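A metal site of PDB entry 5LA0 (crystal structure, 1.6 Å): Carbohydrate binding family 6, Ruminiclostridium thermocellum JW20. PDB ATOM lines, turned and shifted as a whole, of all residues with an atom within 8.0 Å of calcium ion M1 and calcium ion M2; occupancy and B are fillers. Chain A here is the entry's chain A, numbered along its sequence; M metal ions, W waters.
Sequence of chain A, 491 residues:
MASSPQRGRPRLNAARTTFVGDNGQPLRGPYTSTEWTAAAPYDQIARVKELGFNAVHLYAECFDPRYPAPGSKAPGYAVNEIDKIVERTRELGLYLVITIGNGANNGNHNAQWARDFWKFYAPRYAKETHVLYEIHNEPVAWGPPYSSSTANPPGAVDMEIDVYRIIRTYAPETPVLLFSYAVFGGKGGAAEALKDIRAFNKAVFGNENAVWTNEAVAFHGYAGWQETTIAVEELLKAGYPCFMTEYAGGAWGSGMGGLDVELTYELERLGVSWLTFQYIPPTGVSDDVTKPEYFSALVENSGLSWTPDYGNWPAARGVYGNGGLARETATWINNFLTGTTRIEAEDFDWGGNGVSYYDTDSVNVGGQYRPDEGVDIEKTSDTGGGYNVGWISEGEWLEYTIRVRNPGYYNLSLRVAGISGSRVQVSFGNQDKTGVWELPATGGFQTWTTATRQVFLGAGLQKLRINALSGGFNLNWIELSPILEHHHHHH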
ATOM      1  N   ASN A 353      -2.507  -8.286  -7.788  1.00  0.00           N
ATOM      2  CA  ASN A 353      -2.446  -6.856  -7.768  1.00  0.00           C
ATOM      3  C   ASN A 353      -0.991  -6.421  -7.800  1.00  0.00           C
ATOM      4  O   ASN A 353      -0.160  -6.815  -6.961  1.00  0.00           O
ATOM      5  CB  ASN A 353      -3.155  -6.325  -6.526  1.00  0.00           C
ATOM      6  CG  ASN A 353      -3.857  -4.994  -6.774  1.00  0.00           C
ATOM      7  OD1 ASN A 353      -3.504  -4.259  -7.690  1.00  0.00           O
ATOM      8  ND2 ASN A 353      -4.850  -4.677  -5.935  1.00  0.00           N
ATOM      9  N   TYR A 357      -2.693  -7.167 -12.893  1.00  0.00           N
ATOM     10  CA  TYR A 357      -3.544  -5.985 -12.927  1.00  0.00           C
ATOM     11  C   TYR A 357      -3.085  -5.074 -11.799  1.00  0.00           C
ATOM     12  O   TYR A 357      -2.353  -5.519 -10.908  1.00  0.00           O
ATOM     13  CB  TYR A 357      -5.016  -6.360 -12.717  1.00  0.00           C
ATOM     14  CG  TYR A 357      -5.319  -7.116 -11.424  1.00  0.00           C
ATOM     15  CD1 TYR A 357      -5.553  -6.432 -10.213  1.00  0.00           C
ATOM     16  CD2 TYR A 357      -5.352  -8.496 -11.401  1.00  0.00           C
ATOM     17  CE1 TYR A 357      -5.842  -7.117  -9.044  1.00  0.00           C
ATOM     18  CE2 TYR A 357      -5.623  -9.183 -10.220  1.00  0.00           C
ATOM     19  CZ  TYR A 357      -5.865  -8.471  -9.051  1.00  0.00           C
ATOM     20  OH  TYR A 357      -6.129  -9.145  -7.870  1.00  0.00           O
ATOM     21  N   TYR A 358      -3.528  -3.838 -11.814  1.00  0.00           N
ATOM     22  CA  TYR A 358      -3.379  -2.960 -10.681  1.00  0.00           C
ATOM     23  C   TYR A 358      -4.742  -2.357 -10.405  1.00  0.00           C
ATOM     24  O   TYR A 358      -5.365  -1.754 -11.300  1.00  0.00           O
ATOM     25  CB  TYR A 358      -2.343  -1.844 -10.922  1.00  0.00           C
ATOM     26  CG  TYR A 358      -2.313  -0.861  -9.746  1.00  0.00           C
ATOM     27  CD1 TYR A 358      -1.740  -1.214  -8.521  1.00  0.00           C
ATOM     28  CD2 TYR A 358      -2.905   0.381  -9.844  1.00  0.00           C
ATOM     29  CE1 TYR A 358      -1.745  -0.343  -7.440  1.00  0.00           C
ATOM     30  CE2 TYR A 358      -2.922   1.267  -8.774  1.00  0.00           C
ATOM     31  CZ  TYR A 358      -2.337   0.899  -7.581  1.00  0.00           C
ATOM     32  OH  TYR A 358      -2.344   1.771  -6.529  1.00  0.00           O
ATOM     33  N   ASP A 359      -5.206  -2.544  -9.159  1.00  0.00           N
ATOM     34  CA  ASP A 359      -6.471  -2.023  -8.722  1.00  0.00           C
ATOM     35  C   ASP A 359      -6.285  -1.291  -7.416  1.00  0.00           C
ATOM     36  O   ASP A 359      -5.602  -1.782  -6.522  1.00  0.00           O
ATOM     37  CB  ASP A 359      -7.514  -3.128  -8.519  1.00  0.00           C
ATOM     38  CG  ASP A 359      -8.959  -2.576  -8.683  1.00  0.00           C
ATOM     39  OD1 ASP A 359      -9.433  -2.517  -9.864  1.00  0.00           O
ATOM     40  OD2 ASP A 359      -9.588  -2.125  -7.676  1.00  0.00           O
ATOM     41  N   THR A 360      -6.938  -0.141  -7.296  1.00  0.00           N
ATOM     42  CA  THR A 360      -6.796   0.741  -6.135  1.00  0.00           C
ATOM     43  C   THR A 360      -7.316   0.102  -4.844  1.00  0.00           C
ATOM     44  O   THR A 360      -6.843   0.467  -3.768  1.00  0.00           O
ATOM     45  CB  THR A 360      -7.462   2.117  -6.381  1.00  0.00           C
ATOM     46  OG1 THR A 360      -8.887   1.966  -6.626  1.00  0.00           O
ATOM     47  CG2 THR A 360      -6.859   2.736  -7.587  1.00  0.00           C
ATOM     48  N   ASP A 361      -8.265  -0.842  -4.927  1.00  0.00           N
ATOM     49  CA  ASP A 361      -8.781  -1.573  -3.747  1.00  0.00           C
ATOM     50  C   ASP A 361      -8.620  -3.062  -4.005  1.00  0.00           C
ATOM     51  O   ASP A 361      -8.902  -3.554  -5.091  1.00  0.00           O
ATOM     52  CB  ASP A 361     -10.274  -1.300  -3.427  1.00  0.00           C
ATOM     53  CG  ASP A 361     -10.744   0.097  -3.795  1.00  0.00           C
ATOM     54  OD1 ASP A 361     -10.014   1.081  -3.515  1.00  0.00           O
ATOM     55  OD2 ASP A 361     -11.863   0.210  -4.345  1.00  0.00           O
ATOM     56  N   SER A 362      -8.180  -3.789  -2.985  1.00  0.00           N
ATOM     57  CA  SER A 362      -8.025  -5.224  -3.077  1.00  0.00           C
ATOM     58  C   SER A 362      -9.332  -6.016  -3.260  1.00  0.00           C
ATOM     59  O   SER A 362      -9.300  -7.150  -3.676  1.00  0.00           O
ATOM     60  CB  SER A 362      -7.314  -5.717  -1.821  1.00  0.00           C
ATOM     61  OG  SER A 362      -8.056  -5.378  -0.663  1.00  0.00           O
ATOM     62  N   VAL A 363     -10.461  -5.433  -2.896  1.00  0.00           N
ATOM     63  CA  VAL A 363     -11.788  -6.046  -3.040  1.00  0.00           C
ATOM     64  C   VAL A 363     -12.345  -5.816  -4.435  1.00  0.00           C
ATOM     65  O   VAL A 363     -12.157  -4.746  -5.035  1.00  0.00           O
ATOM     66  CB  VAL A 363     -12.756  -5.490  -1.957  1.00  0.00           C
ATOM     67  CG1 VAL A 363     -14.183  -5.992  -2.157  1.00  0.00           C
ATOM     68  CG2 VAL A 363     -12.268  -5.900  -0.575  1.00  0.00           C
ATOM     69  N   ASN A 364     -13.024  -6.840  -4.940  1.00  0.00           N
ATOM     70  CA  ASN A 364     -13.852  -6.758  -6.146  1.00  0.00           C
ATOM     71  C   ASN A 364     -15.237  -6.292  -5.675  1.00  0.00           C
ATOM     72  O   ASN A 364     -16.057  -7.111  -5.216  1.00  0.00           O
ATOM     73  CB  ASN A 364     -13.914  -8.117  -6.830  1.00  0.00           C
ATOM     74  CG  ASN A 364     -14.956  -8.192  -7.944  1.00  0.00           C
ATOM     75  OD1 ASN A 364     -15.678  -7.244  -8.227  1.00  0.00           O
ATOM     76  ND2 ASN A 364     -15.025  -9.362  -8.573  1.00  0.00           N
ATOM     77  N   VAL A 365     -15.485  -4.995  -5.811  1.00  0.00           N
ATOM     78  CA  VAL A 365     -16.702  -4.433  -5.209  1.00  0.00           C
ATOM     79  C   VAL A 365     -17.949  -4.784  -5.944  1.00  0.00           C
ATOM     80  O   VAL A 365     -19.003  -4.712  -5.362  1.00  0.00           O
ATOM     81  CB  VAL A 365     -16.644  -2.925  -4.944  1.00  0.00           C
ATOM     82  CG1 VAL A 365     -15.526  -2.621  -3.960  1.00  0.00           C
ATOM     83  CG2 VAL A 365     -16.492  -2.120  -6.230  1.00  0.00           C
ATOM     84  N   GLY A 366     -17.827  -5.160  -7.210  1.00  0.00           N
ATOM     85  CA  GLY A 366     -18.951  -5.659  -8.003  1.00  0.00           C
ATOM     86  C   GLY A 366     -19.363  -7.078  -7.609  1.00  0.00           C
ATOM     87  O   GLY A 366     -20.520  -7.444  -7.764  1.00  0.00           O
ATOM     88  N   GLU A 373     -10.410 -11.773  -6.576  1.00  0.00           N
ATOM     89  CA  GLU A 373      -9.383 -10.897  -7.124  1.00  0.00           C
ATOM     90  C   GLU A 373      -9.818  -9.454  -6.975  1.00  0.00           C
ATOM     91  O   GLU A 373     -10.948  -9.184  -6.579  1.00  0.00           O
ATOM     92  CB  GLU A 373      -9.070 -11.330  -8.561  1.00  0.00           C
ATOM     93  CG  GLU A 373      -8.232 -12.610  -8.583  1.00  0.00           C
ATOM     94  CD  GLU A 373      -8.280 -13.377  -9.907  1.00  0.00           C
ATOM     95  OE1 GLU A 373      -7.279 -13.295 -10.635  1.00  0.00           O
ATOM     96  OE2 GLU A 373      -9.297 -14.079 -10.208  1.00  0.00           O
ATOM     97  N   GLY A 374      -8.900  -8.532  -7.245  1.00  0.00           N
ATOM     98  CA  GLY A 374      -9.065  -7.096  -6.945  1.00  0.00           C
ATOM     99  C   GLY A 374      -9.769  -6.267  -7.995  1.00  0.00           C
ATOM    100  O   GLY A 374     -10.200  -5.138  -7.710  1.00  0.00           O
ATOM    101  N   VAL A 375      -9.911  -6.812  -9.184  1.00  0.00           N
ATOM    102  CA  VAL A 375     -10.599  -6.129 -10.278  1.00  0.00           C
ATOM    103  C   VAL A 375     -12.109  -6.105 -10.002  1.00  0.00           C
ATOM    104  O   VAL A 375     -12.664  -7.101  -9.583  1.00  0.00           O
ATOM    105  CB  VAL A 375     -10.276  -6.751 -11.653  1.00  0.00           C
ATOM    106  CG1 VAL A 375     -10.973  -5.991 -12.781  1.00  0.00           C
ATOM    107  CG2 VAL A 375      -8.757  -6.715 -11.891  1.00  0.00           C
ATOM    108  N   ASP A 376     -12.748  -4.977 -10.277  1.00  0.00           N
ATOM    109  CA  ASP A 376     -14.166  -4.785  -9.967  1.00  0.00           C
ATOM    110  C   ASP A 376     -14.994  -5.170 -11.187  1.00  0.00           C
ATOM    111  O   ASP A 376     -14.826  -4.579 -12.268  1.00  0.00           O
ATOM    112  CB  ASP A 376     -14.378  -3.339  -9.562  1.00  0.00           C
ATOM    113  CG  ASP A 376     -13.437  -2.929  -8.446  1.00  0.00           C
ATOM    114  OD1 ASP A 376     -13.503  -3.566  -7.360  1.00  0.00           O
ATOM    115  OD2 ASP A 376     -12.553  -2.059  -8.651  1.00  0.00           O
ATOM    116  N   ILE A 377     -15.852  -6.183 -11.017  1.00  0.00           N
ATOM    117  CA  ILE A 377     -16.585  -6.801 -12.107  1.00  0.00           C
ATOM    118  C   ILE A 377     -18.070  -6.902 -11.738  1.00  0.00           C
ATOM    119  O   ILE A 377     -18.435  -7.362 -10.663  1.00  0.00           O
ATOM    120  CB  ILE A 377     -16.060  -8.231 -12.429  1.00  0.00           C
ATOM    121  CG1 ILE A 377     -14.523  -8.227 -12.579  1.00  0.00           C
ATOM    122  CG2 ILE A 377     -16.771  -8.831 -13.648  1.00  0.00           C
ATOM    123  CD1 ILE A 377     -13.902  -9.567 -12.608  1.00  0.00           C
ATOM    124  N   VAL A 389     -15.863  -4.981 -16.642  1.00  0.00           N
ATOM    125  CA  VAL A 389     -15.033  -4.377 -15.639  1.00  0.00           C
ATOM    126  C   VAL A 389     -15.566  -2.968 -15.411  1.00  0.00           C
ATOM    127  O   VAL A 389     -15.856  -2.232 -16.364  1.00  0.00           O
ATOM    128  CB  VAL A 389     -13.525  -4.337 -16.039  1.00  0.00           C
ATOM    129  CG1 VAL A 389     -12.710  -3.530 -15.007  1.00  0.00           C
ATOM    130  CG2 VAL A 389     -12.993  -5.752 -16.231  1.00  0.00           C
ATOM    131  N   GLY A 390     -15.732  -2.609 -14.145  1.00  0.00           N
ATOM    132  CA  GLY A 390     -16.182  -1.267 -13.753  1.00  0.00           C
ATOM    133  C   GLY A 390     -15.336  -0.725 -12.630  1.00  0.00           C
ATOM    134  O   GLY A 390     -14.255  -1.287 -12.307  1.00  0.00           O
ATOM    135  N   TRP A 391     -15.777   0.382 -12.053  1.00  0.00           N
ATOM    136  CA  TRP A 391     -15.032   1.042 -10.966  1.00  0.00           C
ATOM    137  C   TRP A 391     -13.574   1.245 -11.376  1.00  0.00           C
ATOM    138  O   TRP A 391     -12.623   0.896 -10.634  1.00  0.00           O
ATOM    139  CB  TRP A 391     -15.155   0.262  -9.655  1.00  0.00           C
ATOM    140  CG  TRP A 391     -16.556   0.086  -9.142  1.00  0.00           C
ATOM    141  CD1 TRP A 391     -17.183   0.865  -8.228  1.00  0.00           C
ATOM    142  CD2 TRP A 391     -17.533  -0.912  -9.529  1.00  0.00           C
ATOM    143  NE1 TRP A 391     -18.457   0.422  -8.019  1.00  0.00           N
ATOM    144  CE2 TRP A 391     -18.701  -0.671  -8.796  1.00  0.00           C
ATOM    145  CE3 TRP A 391     -17.518  -1.995 -10.422  1.00  0.00           C
ATOM    146  CZ2 TRP A 391     -19.853  -1.458  -8.897  1.00  0.00           C
ATOM    147  CZ3 TRP A 391     -18.659  -2.788 -10.534  1.00  0.00           C
ATOM    148  CH2 TRP A 391     -19.814  -2.497  -9.753  1.00  0.00           C
ATOM    149  N   ILE A 392     -13.401   1.759 -12.584  1.00  0.00           N
ATOM    150  CA  ILE A 392     -12.089   1.966 -13.133  1.00  0.00           C
ATOM    151  C   ILE A 392     -11.610   3.362 -12.710  1.00  0.00           C
ATOM    152  O   ILE A 392     -12.339   4.356 -12.833  1.00  0.00           O
ATOM    153  CB  ILE A 392     -12.068   1.794 -14.657  1.00  0.00           C
ATOM    154  CG1 ILE A 392     -12.629   0.427 -15.027  1.00  0.00           C
ATOM    155  CG2 ILE A 392     -10.647   2.007 -15.170  1.00  0.00           C
ATOM    156  CD1 ILE A 392     -12.537   0.048 -16.488  1.00  0.00           C
ATOM    157  N   SER A 393     -10.393   3.436 -12.193  1.00  0.00           N
ATOM    158  CA  SER A 393      -9.849   4.732 -11.816  1.00  0.00           C
ATOM    159  C   SER A 393      -8.470   4.983 -12.401  1.00  0.00           C
ATOM    160  O   SER A 393      -7.781   4.041 -12.882  1.00  0.00           O
ATOM    161  CB  SER A 393      -9.884   4.888 -10.316  1.00  0.00           C
ATOM    162  OG  SER A 393      -8.889   4.135  -9.754  1.00  0.00           O
ATOM    163  N   GLU A 394      -8.063   6.243 -12.361  1.00  0.00           N
ATOM    164  CA  GLU A 394      -6.786   6.645 -12.957  1.00  0.00           C
ATOM    165  C   GLU A 394      -5.639   5.802 -12.404  1.00  0.00           C
ATOM    166  O   GLU A 394      -5.552   5.613 -11.212  1.00  0.00           O
ATOM    167  CB  GLU A 394      -6.513   8.134 -12.661  1.00  0.00           C
ATOM    168  CG  GLU A 394      -5.295   8.670 -13.381  1.00  0.00           C
ATOM    169  CD  GLU A 394      -4.971  10.131 -13.071  1.00  0.00           C
ATOM    170  OE1 GLU A 394      -5.848  10.878 -12.582  1.00  0.00           O
ATOM    171  OE2 GLU A 394      -3.815  10.548 -13.323  1.00  0.00           O
ATOM    172  N   GLU A 396      -5.156   2.545 -12.822  1.00  0.00           N
ATOM    173  CA  GLU A 396      -5.471   1.130 -12.903  1.00  0.00           C
ATOM    174  C   GLU A 396      -4.991   0.577 -14.247  1.00  0.00           C
ATOM    175  O   GLU A 396      -4.851   1.313 -15.236  1.00  0.00           O
ATOM    176  CB  GLU A 396      -6.930   0.838 -12.620  1.00  0.00           C
ATOM    177  CG  GLU A 396      -7.308   1.129 -11.178  1.00  0.00           C
ATOM    178  CD  GLU A 396      -8.646   0.565 -10.720  1.00  0.00           C
ATOM    179  OE1 GLU A 396      -9.551   0.332 -11.575  1.00  0.00           O
ATOM    180  OE2 GLU A 396      -8.794   0.383  -9.469  1.00  0.00           O
ATOM    181  N   TRP A 397      -4.687  -0.712 -14.254  1.00  0.00           N
ATOM    182  CA  TRP A 397      -4.335  -1.405 -15.490  1.00  0.00           C
ATOM    183  C   TRP A 397      -4.666  -2.889 -15.435  1.00  0.00           C
ATOM    184  O   TRP A 397      -4.908  -3.448 -14.366  1.00  0.00           O
ATOM    185  CB  TRP A 397      -2.871  -1.156 -15.876  1.00  0.00           C
ATOM    186  CG  TRP A 397      -1.813  -1.429 -14.816  1.00  0.00           C
ATOM    187  CD1 TRP A 397      -1.218  -0.515 -14.010  1.00  0.00           C
ATOM    188  CD2 TRP A 397      -1.181  -2.689 -14.519  1.00  0.00           C
ATOM    189  NE1 TRP A 397      -0.232  -1.108 -13.230  1.00  0.00           N
ATOM    190  CE2 TRP A 397      -0.183  -2.441 -13.545  1.00  0.00           C
ATOM    191  CE3 TRP A 397      -1.329  -4.000 -15.008  1.00  0.00           C
ATOM    192  CZ2 TRP A 397       0.609  -3.454 -13.006  1.00  0.00           C
ATOM    193  CZ3 TRP A 397      -0.525  -4.996 -14.520  1.00  0.00           C
ATOM    194  CH2 TRP A 397       0.441  -4.722 -13.505  1.00  0.00           C
ATOM    195  N   LEU A 398      -4.741  -3.478 -16.613  1.00  0.00           N
ATOM    196  CA  LEU A 398      -5.185  -4.841 -16.844  1.00  0.00           C
ATOM    197  C   LEU A 398      -4.336  -5.445 -17.931  1.00  0.00           C
ATOM    198  O   LEU A 398      -4.111  -4.803 -18.948  1.00  0.00           O
ATOM    199  CB  LEU A 398      -6.646  -4.895 -17.283  1.00  0.00           C
ATOM    200  CG  LEU A 398      -7.666  -4.210 -16.393  1.00  0.00           C
ATOM    201  CD1 LEU A 398      -8.882  -3.856 -17.183  1.00  0.00           C
ATOM    202  CD2 LEU A 398      -8.051  -5.133 -15.257  1.00  0.00           C
HETATM  203 CA    CA M   1     -11.015  -0.714  -9.808  1.00  0.00          CA
HETATM  204 CA    CA M   2     -11.163  -3.329  -6.494  1.00  0.00          CA
HETATM  205  O   HOH W   1     -11.837  -2.220 -11.626  1.00  0.00           O
HETATM  206  O   HOH W   2     -11.239   0.676  -7.848  1.00  0.00           O
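The backbone NH (N) of Asp 359 lies within hydrogen-bond range of the side-chain amide oxygen (OD1) of Asn 353, at 2.8 Å.
The backbone carbonyl oxygen of Asp 376 sits at hydrogen-bond distance from the backbone NH of Gly 390.
OD1 of Asp 376 sits close to N of Val 365 (2.9 Å).
N of Gly 374 is in hydrogen-bond range of OH of Tyr 357, 2.9 Å away.
OE2 of Glu 396 lies close to N of Thr 360 (2.9 Å).
OE1 of Glu 396 sits close to N of Ser 393, at 3.3 Å.
The side-chain carboxylate (OD1) of Asp 361 sits close to the side-chain hydroxyl (OG1) of Thr 360 (3.4 Å).
Along chain A the residues within 4 Å of calcium ion M2 span positions 359 to 376.
Calcium ion M1 is bound by the side-chain carboxylate (OD2) of Asp 376, the side-chain carboxylate (OD1) of Asp 359, water W2, the backbone carbonyl oxygen (O) of Trp 391, water W1, the side-chain carboxylate (OE2) of Glu 396 and the side-chain carboxylate (OE1) of Glu 396.
Slightly farther from calcium ion M1 lies OD2 of Asp 359 (2.9 Å).
Calcium ion M2 is bound by O of Val 363 (2.3 Å), OD2 of Asp 359 (2.3 Å), O of Gly 374 (2.4 Å), OD1 of Asp 376 (2.5 Å), O of Asp 361 (2.7 Å) and OD2 of Asp 376 (2.9 Å).
Water W1 bridges O of Gly 390 (2.7 Å) and N of Asp 376 (3.2 Å).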
